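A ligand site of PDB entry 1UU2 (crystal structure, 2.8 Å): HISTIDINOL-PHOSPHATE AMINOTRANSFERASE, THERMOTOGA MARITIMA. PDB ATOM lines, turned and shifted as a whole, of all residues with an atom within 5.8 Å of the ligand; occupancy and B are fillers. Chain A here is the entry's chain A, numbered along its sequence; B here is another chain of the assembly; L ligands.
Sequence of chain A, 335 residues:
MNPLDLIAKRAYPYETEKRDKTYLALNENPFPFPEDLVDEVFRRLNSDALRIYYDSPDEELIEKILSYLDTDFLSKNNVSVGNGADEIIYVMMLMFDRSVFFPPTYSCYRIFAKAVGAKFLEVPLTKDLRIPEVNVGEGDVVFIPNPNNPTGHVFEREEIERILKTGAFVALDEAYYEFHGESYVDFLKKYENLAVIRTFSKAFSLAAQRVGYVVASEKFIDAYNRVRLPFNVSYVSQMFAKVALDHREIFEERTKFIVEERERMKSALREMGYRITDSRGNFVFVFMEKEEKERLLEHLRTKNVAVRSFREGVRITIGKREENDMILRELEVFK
N of Ala 85 sits at hydrogen-bond distance from O4 of the ligand (2.6 Å).
The guanidinium group of Arg 210 lies within salt-bridge range of an oxygen (O5) of the ligand.
An oxygen (O1) of the ligand is in hydrogen-bond range of the side-chain hydroxyl (OH) of Tyr 176, 2.7 Å away.
An oxygen (O5) of the ligand sits at hydrogen-bond distance from the side-chain hydroxyl (OH) of Tyr 53 of chain B, 2.7 Å away.
OD2 of Asp 173 sits at hydrogen-bond distance from N1 of the ligand (2.7 Å).
The side-chain hydroxyl of Thr 199 is in hydrogen-bond range of an oxygen (O4) of the ligand (2.8 Å).
The side-chain hydroxyl (OG) of Ser 201 sits at hydrogen-bond distance from an oxygen (O5) of the ligand (2.8 Å).
N of Asp 86 sits at hydrogen-bond distance from O3 of the ligand.
ND2 of Asn 149 is in hydrogen-bond range of O1 of the ligand, at 3.1 Å.
NH2 of Arg 210 lies within salt-bridge range of OD2 of Asp 86 (3.5 Å).
The backbone carbonyl oxygen (O) of Arg 210 lies within hydrogen-bond range of the backbone NH (N) of Gly 84.
OH of Tyr 176 lies within hydrogen-bond range of ND2 of Asn 149, at 2.9 Å.
The side-chain amide oxygen of Asn 27 lies within hydrogen-bond range of the side-chain hydroxyl of Tyr 176 (2.9 Å).
The side-chain hydroxyl of Tyr 53 of chain B is in hydrogen-bond range of the side-chain amino group of Lys 202 (2.9 Å).
The backbone NH of Ala 175 sits at hydrogen-bond distance from the side-chain carboxylate of Asp 173, 3.0 Å away.
The side-chain carboxylate (OD2) of Asp 173 is in hydrogen-bond range of the side-chain hydroxyl (OH) of Tyr 109 (3.1 Å).
The backbone NH (N) of Ser 201 is in hydrogen-bond range of the side-chain hydroxyl (OG1) of Thr 199.
Merely in contact with the ligand: Gly 84 (3.5 Å), Tyr 106 (3.5 Å), Ala 175 (3.6 Å) and Lys 202 (3.3 Å).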
ATOM      1  N   ASN A  27     -19.561  -6.784 -24.103  1.00  0.00           N
ATOM      2  CA  ASN A  27     -20.899  -7.158 -23.659  1.00  0.00           C
ATOM      3  C   ASN A  27     -20.937  -7.606 -22.197  1.00  0.00           C
ATOM      4  O   ASN A  27     -21.790  -8.396 -21.804  1.00  0.00           O
ATOM      5  CB  ASN A  27     -21.461  -8.256 -24.551  1.00  0.00           C
ATOM      6  CG  ASN A  27     -21.935  -7.722 -25.883  1.00  0.00           C
ATOM      7  OD1 ASN A  27     -22.219  -8.484 -26.807  1.00  0.00           O
ATOM      8  ND2 ASN A  27     -22.038  -6.408 -25.988  1.00  0.00           N
ATOM      9  N   ASN A  83     -17.158 -25.111 -19.162  1.00  0.00           N
ATOM     10  CA  ASN A  83     -16.328 -24.023 -18.658  1.00  0.00           C
ATOM     11  C   ASN A  83     -16.689 -22.763 -19.411  1.00  0.00           C
ATOM     12  O   ASN A  83     -15.893 -22.231 -20.184  1.00  0.00           O
ATOM     13  CB  ASN A  83     -14.857 -24.346 -18.850  1.00  0.00           C
ATOM     14  CG  ASN A  83     -13.956 -23.182 -18.479  1.00  0.00           C
ATOM     15  OD1 ASN A  83     -13.945 -22.732 -17.337  1.00  0.00           O
ATOM     16  ND2 ASN A  83     -13.202 -22.693 -19.444  1.00  0.00           N
ATOM     17  N   GLY A  84     -17.897 -22.274 -19.175  1.00  0.00           N
ATOM     18  CA  GLY A  84     -18.363 -21.083 -19.861  1.00  0.00           C
ATOM     19  C   GLY A  84     -18.998 -21.531 -21.172  1.00  0.00           C
ATOM     20  O   GLY A  84     -18.672 -22.608 -21.673  1.00  0.00           O
ATOM     21  N   ALA A  85     -19.884 -20.716 -21.715  1.00  0.00           N
ATOM     22  CA  ALA A  85     -20.547 -21.041 -22.966  1.00  0.00           C
ATOM     23  C   ALA A  85     -19.536 -21.385 -24.069  1.00  0.00           C
ATOM     24  O   ALA A  85     -19.824 -22.171 -24.965  1.00  0.00           O
ATOM     25  CB  ALA A  85     -21.425 -19.895 -23.412  1.00  0.00           C
ATOM     26  N   ASP A  86     -18.351 -20.790 -23.996  1.00  0.00           N
ATOM     27  CA  ASP A  86     -17.324 -21.053 -24.990  1.00  0.00           C
ATOM     28  C   ASP A  86     -16.976 -22.529 -25.113  1.00  0.00           C
ATOM     29  O   ASP A  86     -17.036 -23.091 -26.207  1.00  0.00           O
ATOM     30  CB  ASP A  86     -16.043 -20.256 -24.698  1.00  0.00           C
ATOM     31  CG  ASP A  86     -16.108 -18.835 -25.243  1.00  0.00           C
ATOM     32  OD1 ASP A  86     -16.904 -18.581 -26.174  1.00  0.00           O
ATOM     33  OD2 ASP A  86     -15.336 -17.979 -24.756  1.00  0.00           O
ATOM     34  N   GLU A  87     -16.622 -23.169 -24.004  1.00  0.00           N
ATOM     35  CA  GLU A  87     -16.272 -24.587 -24.050  1.00  0.00           C
ATOM     36  C   GLU A  87     -17.398 -25.420 -24.660  1.00  0.00           C
ATOM     37  O   GLU A  87     -17.133 -26.463 -25.252  1.00  0.00           O
ATOM     38  CB  GLU A  87     -15.941 -25.117 -22.658  1.00  0.00           C
ATOM     39  CG  GLU A  87     -15.340 -26.520 -22.684  1.00  0.00           C
ATOM     40  CD  GLU A  87     -15.181 -27.127 -21.302  1.00  0.00           C
ATOM     41  OE1 GLU A  87     -16.192 -27.185 -20.571  1.00  0.00           O
ATOM     42  OE2 GLU A  87     -14.053 -27.535 -20.958  1.00  0.00           O
ATOM     43  N   ILE A  89     -19.360 -24.494 -27.117  1.00  0.00           N
ATOM     44  CA  ILE A  89     -19.200 -24.288 -28.538  1.00  0.00           C
ATOM     45  C   ILE A  89     -17.998 -25.113 -28.989  1.00  0.00           C
ATOM     46  O   ILE A  89     -18.061 -25.876 -29.952  1.00  0.00           O
ATOM     47  CB  ILE A  89     -18.917 -22.802 -28.853  1.00  0.00           C
ATOM     48  CG1 ILE A  89     -20.045 -21.917 -28.311  1.00  0.00           C
ATOM     49  CG2 ILE A  89     -18.712 -22.607 -30.349  1.00  0.00           C
ATOM     50  CD1 ILE A  89     -21.402 -22.198 -28.923  1.00  0.00           C
ATOM     51  N   TYR A 106     -21.048 -14.425 -33.881  1.00  0.00           N
ATOM     52  CA  TYR A 106     -20.068 -14.455 -32.803  1.00  0.00           C
ATOM     53  C   TYR A 106     -18.699 -14.763 -33.391  1.00  0.00           C
ATOM     54  O   TYR A 106     -18.506 -15.797 -34.023  1.00  0.00           O
ATOM     55  CB  TYR A 106     -20.472 -15.499 -31.757  1.00  0.00           C
ATOM     56  CG  TYR A 106     -19.552 -15.587 -30.555  1.00  0.00           C
ATOM     57  CD1 TYR A 106     -18.995 -14.440 -29.995  1.00  0.00           C
ATOM     58  CD2 TYR A 106     -19.251 -16.822 -29.981  1.00  0.00           C
ATOM     59  CE1 TYR A 106     -18.167 -14.515 -28.884  1.00  0.00           C
ATOM     60  CE2 TYR A 106     -18.420 -16.911 -28.860  1.00  0.00           C
ATOM     61  CZ  TYR A 106     -17.880 -15.747 -28.323  1.00  0.00           C
ATOM     62  OH  TYR A 106     -17.045 -15.818 -27.219  1.00  0.00           O
ATOM     63  N   TYR A 109     -16.668 -18.216 -33.202  1.00  0.00           N
ATOM     64  CA  TYR A 109     -17.141 -19.395 -33.924  1.00  0.00           C
ATOM     65  C   TYR A 109     -16.104 -19.804 -34.963  1.00  0.00           C
ATOM     66  O   TYR A 109     -15.830 -20.990 -35.156  1.00  0.00           O
ATOM     67  CB  TYR A 109     -18.467 -19.123 -34.630  1.00  0.00           C
ATOM     68  CG  TYR A 109     -19.681 -19.028 -33.730  1.00  0.00           C
ATOM     69  CD1 TYR A 109     -19.732 -19.736 -32.535  1.00  0.00           C
ATOM     70  CD2 TYR A 109     -20.791 -18.296 -34.116  1.00  0.00           C
ATOM     71  CE1 TYR A 109     -20.868 -19.722 -31.739  1.00  0.00           C
ATOM     72  CE2 TYR A 109     -21.947 -18.284 -33.328  1.00  0.00           C
ATOM     73  CZ  TYR A 109     -21.976 -18.993 -32.142  1.00  0.00           C
ATOM     74  OH  TYR A 109     -23.102 -18.983 -31.356  1.00  0.00           O
ATOM     75  N   PRO A 145     -26.626 -18.028 -32.798  1.00  0.00           N
ATOM     76  CA  PRO A 145     -26.834 -17.241 -31.586  1.00  0.00           C
ATOM     77  C   PRO A 145     -28.133 -16.444 -31.770  1.00  0.00           C
ATOM     78  O   PRO A 145     -28.384 -15.904 -32.840  1.00  0.00           O
ATOM     79  CB  PRO A 145     -25.596 -16.347 -31.552  1.00  0.00           C
ATOM     80  CG  PRO A 145     -25.266 -16.170 -33.005  1.00  0.00           C
ATOM     81  CD  PRO A 145     -25.449 -17.572 -33.539  1.00  0.00           C
ATOM     82  N   PRO A 147     -30.785 -13.947 -29.164  1.00  0.00           N
ATOM     83  CA  PRO A 147     -30.365 -12.814 -30.012  1.00  0.00           C
ATOM     84  C   PRO A 147     -28.981 -12.995 -30.625  1.00  0.00           C
ATOM     85  O   PRO A 147     -28.072 -13.565 -30.012  1.00  0.00           O
ATOM     86  CB  PRO A 147     -30.398 -11.630 -29.048  1.00  0.00           C
ATOM     87  CG  PRO A 147     -31.500 -11.995 -28.127  1.00  0.00           C
ATOM     88  CD  PRO A 147     -31.232 -13.459 -27.852  1.00  0.00           C
ATOM     89  N   ASN A 149     -25.252 -11.940 -32.464  1.00  0.00           N
ATOM     90  CA  ASN A 149     -24.130 -11.075 -32.116  1.00  0.00           C
ATOM     91  C   ASN A 149     -23.521 -10.813 -33.484  1.00  0.00           C
ATOM     92  O   ASN A 149     -23.360 -11.764 -34.256  1.00  0.00           O
ATOM     93  CB  ASN A 149     -23.129 -11.823 -31.235  1.00  0.00           C
ATOM     94  CG  ASN A 149     -22.181 -10.889 -30.501  1.00  0.00           C
ATOM     95  OD1 ASN A 149     -21.628  -9.955 -31.084  1.00  0.00           O
ATOM     96  ND2 ASN A 149     -21.983 -11.150 -29.223  1.00  0.00           N
ATOM     97  N   ASP A 173     -27.526 -20.602 -29.611  1.00  0.00           N
ATOM     98  CA  ASP A 173     -26.755 -19.916 -28.590  1.00  0.00           C
ATOM     99  C   ASP A 173     -27.553 -18.799 -27.933  1.00  0.00           C
ATOM    100  O   ASP A 173     -27.563 -17.673 -28.433  1.00  0.00           O
ATOM    101  CB  ASP A 173     -25.481 -19.350 -29.213  1.00  0.00           C
ATOM    102  CG  ASP A 173     -24.525 -18.796 -28.183  1.00  0.00           C
ATOM    103  OD1 ASP A 173     -24.973 -18.036 -27.304  1.00  0.00           O
ATOM    104  OD2 ASP A 173     -23.318 -19.109 -28.278  1.00  0.00           O
ATOM    105  N   ALA A 175     -27.020 -16.856 -25.429  1.00  0.00           N
ATOM    106  CA  ALA A 175     -26.137 -16.154 -24.505  1.00  0.00           C
ATOM    107  C   ALA A 175     -26.740 -14.828 -24.060  1.00  0.00           C
ATOM    108  O   ALA A 175     -26.260 -14.218 -23.098  1.00  0.00           O
ATOM    109  CB  ALA A 175     -24.780 -15.921 -25.161  1.00  0.00           C
ATOM    110  N   TYR A 176     -27.789 -14.382 -24.734  1.00  0.00           N
ATOM    111  CA  TYR A 176     -28.430 -13.114 -24.388  1.00  0.00           C
ATOM    112  C   TYR A 176     -29.913 -13.247 -24.077  1.00  0.00           C
ATOM    113  O   TYR A 176     -30.667 -12.286 -24.190  1.00  0.00           O
ATOM    114  CB  TYR A 176     -28.231 -12.103 -25.516  1.00  0.00           C
ATOM    115  CG  TYR A 176     -26.779 -11.820 -25.803  1.00  0.00           C
ATOM    116  CD1 TYR A 176     -25.993 -11.105 -24.893  1.00  0.00           C
ATOM    117  CD2 TYR A 176     -26.162 -12.333 -26.947  1.00  0.00           C
ATOM    118  CE1 TYR A 176     -24.644 -10.922 -25.117  1.00  0.00           C
ATOM    119  CE2 TYR A 176     -24.799 -12.147 -27.170  1.00  0.00           C
ATOM    120  CZ  TYR A 176     -24.054 -11.447 -26.250  1.00  0.00           C
ATOM    121  OH  TYR A 176     -22.704 -11.275 -26.448  1.00  0.00           O
ATOM    122  N   ARG A 198     -26.702 -21.610 -22.763  1.00  0.00           N
ATOM    123  CA  ARG A 198     -26.856 -20.441 -21.893  1.00  0.00           C
ATOM    124  C   ARG A 198     -25.573 -20.164 -21.135  1.00  0.00           C
ATOM    125  O   ARG A 198     -24.630 -20.963 -21.176  1.00  0.00           O
ATOM    126  CB  ARG A 198     -27.980 -20.679 -20.888  1.00  0.00           C
ATOM    127  CG  ARG A 198     -29.355 -20.956 -21.466  1.00  0.00           C
ATOM    128  CD  ARG A 198     -29.972 -19.709 -22.063  1.00  0.00           C
ATOM    129  NE  ARG A 198     -31.399 -19.864 -22.299  1.00  0.00           N
ATOM    130  CZ  ARG A 198     -32.304 -20.090 -21.342  1.00  0.00           C
ATOM    131  NH1 ARG A 198     -31.915 -20.172 -20.074  1.00  0.00           N
ATOM    132  NH2 ARG A 198     -33.589 -20.212 -21.646  1.00  0.00           N
ATOM    133  N   THR A 199     -25.547 -19.029 -20.438  1.00  0.00           N
ATOM    134  CA  THR A 199     -24.384 -18.628 -19.656  1.00  0.00           C
ATOM    135  C   THR A 199     -24.749 -17.793 -18.449  1.00  0.00           C
ATOM    136  O   THR A 199     -25.858 -17.248 -18.362  1.00  0.00           O
ATOM    137  CB  THR A 199     -23.417 -17.794 -20.502  1.00  0.00           C
ATOM    138  OG1 THR A 199     -22.372 -17.279 -19.668  1.00  0.00           O
ATOM    139  CG2 THR A 199     -24.152 -16.641 -21.164  1.00  0.00           C
ATOM    140  N   PHE A 200     -23.815 -17.684 -17.519  1.00  0.00           N
ATOM    141  CA  PHE A 200     -24.016 -16.893 -16.313  1.00  0.00           C
ATOM    142  C   PHE A 200     -23.158 -15.637 -16.400  1.00  0.00           C
ATOM    143  O   PHE A 200     -23.258 -14.745 -15.554  1.00  0.00           O
ATOM    144  CB  PHE A 200     -23.609 -17.668 -15.063  1.00  0.00           C
ATOM    145  CG  PHE A 200     -24.531 -18.796 -14.708  1.00  0.00           C
ATOM    146  CD1 PHE A 200     -24.412 -20.032 -15.336  1.00  0.00           C
ATOM    147  CD2 PHE A 200     -25.513 -18.621 -13.744  1.00  0.00           C
ATOM    148  CE1 PHE A 200     -25.268 -21.066 -15.005  1.00  0.00           C
ATOM    149  CE2 PHE A 200     -26.368 -19.654 -13.413  1.00  0.00           C
ATOM    150  CZ  PHE A 200     -26.246 -20.877 -14.043  1.00  0.00           C
ATOM    151  N   SER A 201     -22.347 -15.570 -17.441  1.00  0.00           N
ATOM    152  CA  SER A 201     -21.424 -14.460 -17.644  1.00  0.00           C
ATOM    153  C   SER A 201     -22.002 -13.071 -17.916  1.00  0.00           C
ATOM    154  O   SER A 201     -21.462 -12.070 -17.445  1.00  0.00           O
ATOM    155  CB  SER A 201     -20.450 -14.827 -18.770  1.00  0.00           C
ATOM    156  OG  SER A 201     -19.761 -16.026 -18.455  1.00  0.00           O
ATOM    157  N   LYS A 202     -23.092 -13.009 -18.663  1.00  0.00           N
ATOM    158  CA  LYS A 202     -23.676 -11.721 -19.015  1.00  0.00           C
ATOM    159  C   LYS A 202     -24.673 -11.171 -17.995  1.00  0.00           C
ATOM    160  O   LYS A 202     -24.519 -10.059 -17.504  1.00  0.00           O
ATOM    161  CB  LYS A 202     -24.356 -11.826 -20.373  1.00  0.00           C
ATOM    162  CG  LYS A 202     -23.802 -12.953 -21.270  1.00  0.00           C
ATOM    163  CD  LYS A 202     -22.814 -12.471 -22.331  1.00  0.00           C
ATOM    164  CE  LYS A 202     -21.401 -12.306 -21.807  1.00  0.00           C
ATOM    165  NZ  LYS A 202     -20.438 -12.061 -22.933  1.00  0.00           N
ATOM    166  N   ALA A 207     -18.838 -13.484 -15.473  1.00  0.00           N
ATOM    167  CA  ALA A 207     -18.004 -13.774 -16.632  1.00  0.00           C
ATOM    168  C   ALA A 207     -16.592 -14.220 -16.253  1.00  0.00           C
ATOM    169  O   ALA A 207     -15.927 -14.909 -17.027  1.00  0.00           O
ATOM    170  CB  ALA A 207     -17.937 -12.556 -17.540  1.00  0.00           C
ATOM    171  N   ARG A 210     -16.389 -18.242 -15.553  1.00  0.00           N
ATOM    172  CA  ARG A 210     -16.666 -19.170 -16.638  1.00  0.00           C
ATOM    173  C   ARG A 210     -17.638 -20.340 -16.351  1.00  0.00           C
ATOM    174  O   ARG A 210     -17.205 -21.466 -16.081  1.00  0.00           O
ATOM    175  CB  ARG A 210     -15.338 -19.755 -17.125  1.00  0.00           C
ATOM    176  CG  ARG A 210     -14.155 -18.787 -16.981  1.00  0.00           C
ATOM    177  CD  ARG A 210     -14.280 -17.564 -17.866  1.00  0.00           C
ATOM    178  NE  ARG A 210     -14.393 -17.939 -19.279  1.00  0.00           N
ATOM    179  CZ  ARG A 210     -15.508 -17.841 -19.995  1.00  0.00           C
ATOM    180  NH1 ARG A 210     -16.621 -17.381 -19.445  1.00  0.00           N
ATOM    181  NH2 ARG A 210     -15.513 -18.225 -21.263  1.00  0.00           N
ATOM    182  N   VAL A 211     -18.942 -20.088 -16.439  1.00  0.00           N
ATOM    183  CA  VAL A 211     -19.923 -21.145 -16.213  1.00  0.00           C
ATOM    184  C   VAL A 211     -21.093 -21.052 -17.189  1.00  0.00           C
ATOM    185  O   VAL A 211     -21.751 -20.031 -17.304  1.00  0.00           O
ATOM    186  CB  VAL A 211     -20.482 -21.096 -14.780  1.00  0.00           C
ATOM    187  CG1 VAL A 211     -21.360 -22.316 -14.525  1.00  0.00           C
ATOM    188  CG2 VAL A 211     -19.341 -21.023 -13.765  1.00  0.00           C
ATOM    189  N   GLY A 212     -21.345 -22.150 -17.908  1.00  0.00           N
ATOM    190  CA  GLY A 212     -22.426 -22.181 -18.878  1.00  0.00           C
ATOM    191  C   GLY A 212     -23.125 -23.525 -18.879  1.00  0.00           C
ATOM    192  O   GLY A 212     -22.613 -24.493 -18.294  1.00  0.00           O
ATOM    193  N   TYR B  53     -14.053 -10.188 -18.200  1.00  0.00           N
ATOM    194  CA  TYR B  53     -13.345 -11.367 -18.688  1.00  0.00           C
ATOM    195  C   TYR B  53     -11.905 -11.269 -18.200  1.00  0.00           C
ATOM    196  O   TYR B  53     -11.058 -10.634 -18.810  1.00  0.00           O
ATOM    197  CB  TYR B  53     -13.440 -11.430 -20.218  1.00  0.00           C
ATOM    198  CG  TYR B  53     -14.749 -12.033 -20.696  1.00  0.00           C
ATOM    199  CD1 TYR B  53     -14.935 -13.411 -20.707  1.00  0.00           C
ATOM    200  CD2 TYR B  53     -15.823 -11.221 -21.035  1.00  0.00           C
ATOM    201  CE1 TYR B  53     -16.168 -13.976 -21.042  1.00  0.00           C
ATOM    202  CE2 TYR B  53     -17.067 -11.772 -21.356  1.00  0.00           C
ATOM    203  CZ  TYR B  53     -17.219 -13.144 -21.358  1.00  0.00           C
ATOM    204  OH  TYR B  53     -18.439 -13.700 -21.705  1.00  0.00           O
HETATM  205  N1  LIG L   1     -21.988 -17.001 -27.188  1.00  0.00           N
HETATM  206  C1  LIG L   1     -22.074 -15.701 -27.514  1.00  0.00           C
HETATM  207  C2  LIG L   1     -23.055 -15.248 -28.586  1.00  0.00           C
HETATM  208  C3  LIG L   1     -21.249 -14.774 -26.870  1.00  0.00           C
HETATM  209  O1  LIG L   1     -21.333 -13.456 -27.181  1.00  0.00           O
HETATM  210  C4  LIG L   1     -20.358 -15.217 -25.906  1.00  0.00           C
HETATM  211  C5  LIG L   1     -19.442 -14.202 -25.198  1.00  0.00           C
HETATM  212  C6  LIG L   1     -20.294 -16.573 -25.594  1.00  0.00           C
HETATM  213  C7  LIG L   1     -21.139 -17.438 -26.266  1.00  0.00           C
HETATM  214  C8  LIG L   1     -19.357 -17.196 -24.545  1.00  0.00           C
HETATM  215  O2  LIG L   1     -19.631 -16.666 -23.246  1.00  0.00           O
HETATM  216  P1  LIG L   1     -19.129 -17.435 -21.920  1.00  0.00           P
HETATM  217  O3  LIG L   1     -17.934 -18.413 -22.357  1.00  0.00           O
HETATM  218  O4  LIG L   1     -20.244 -18.156 -21.252  1.00  0.00           O
HETATM  219  O5  LIG L   1     -18.484 -16.302 -20.978  1.00  0.00           O
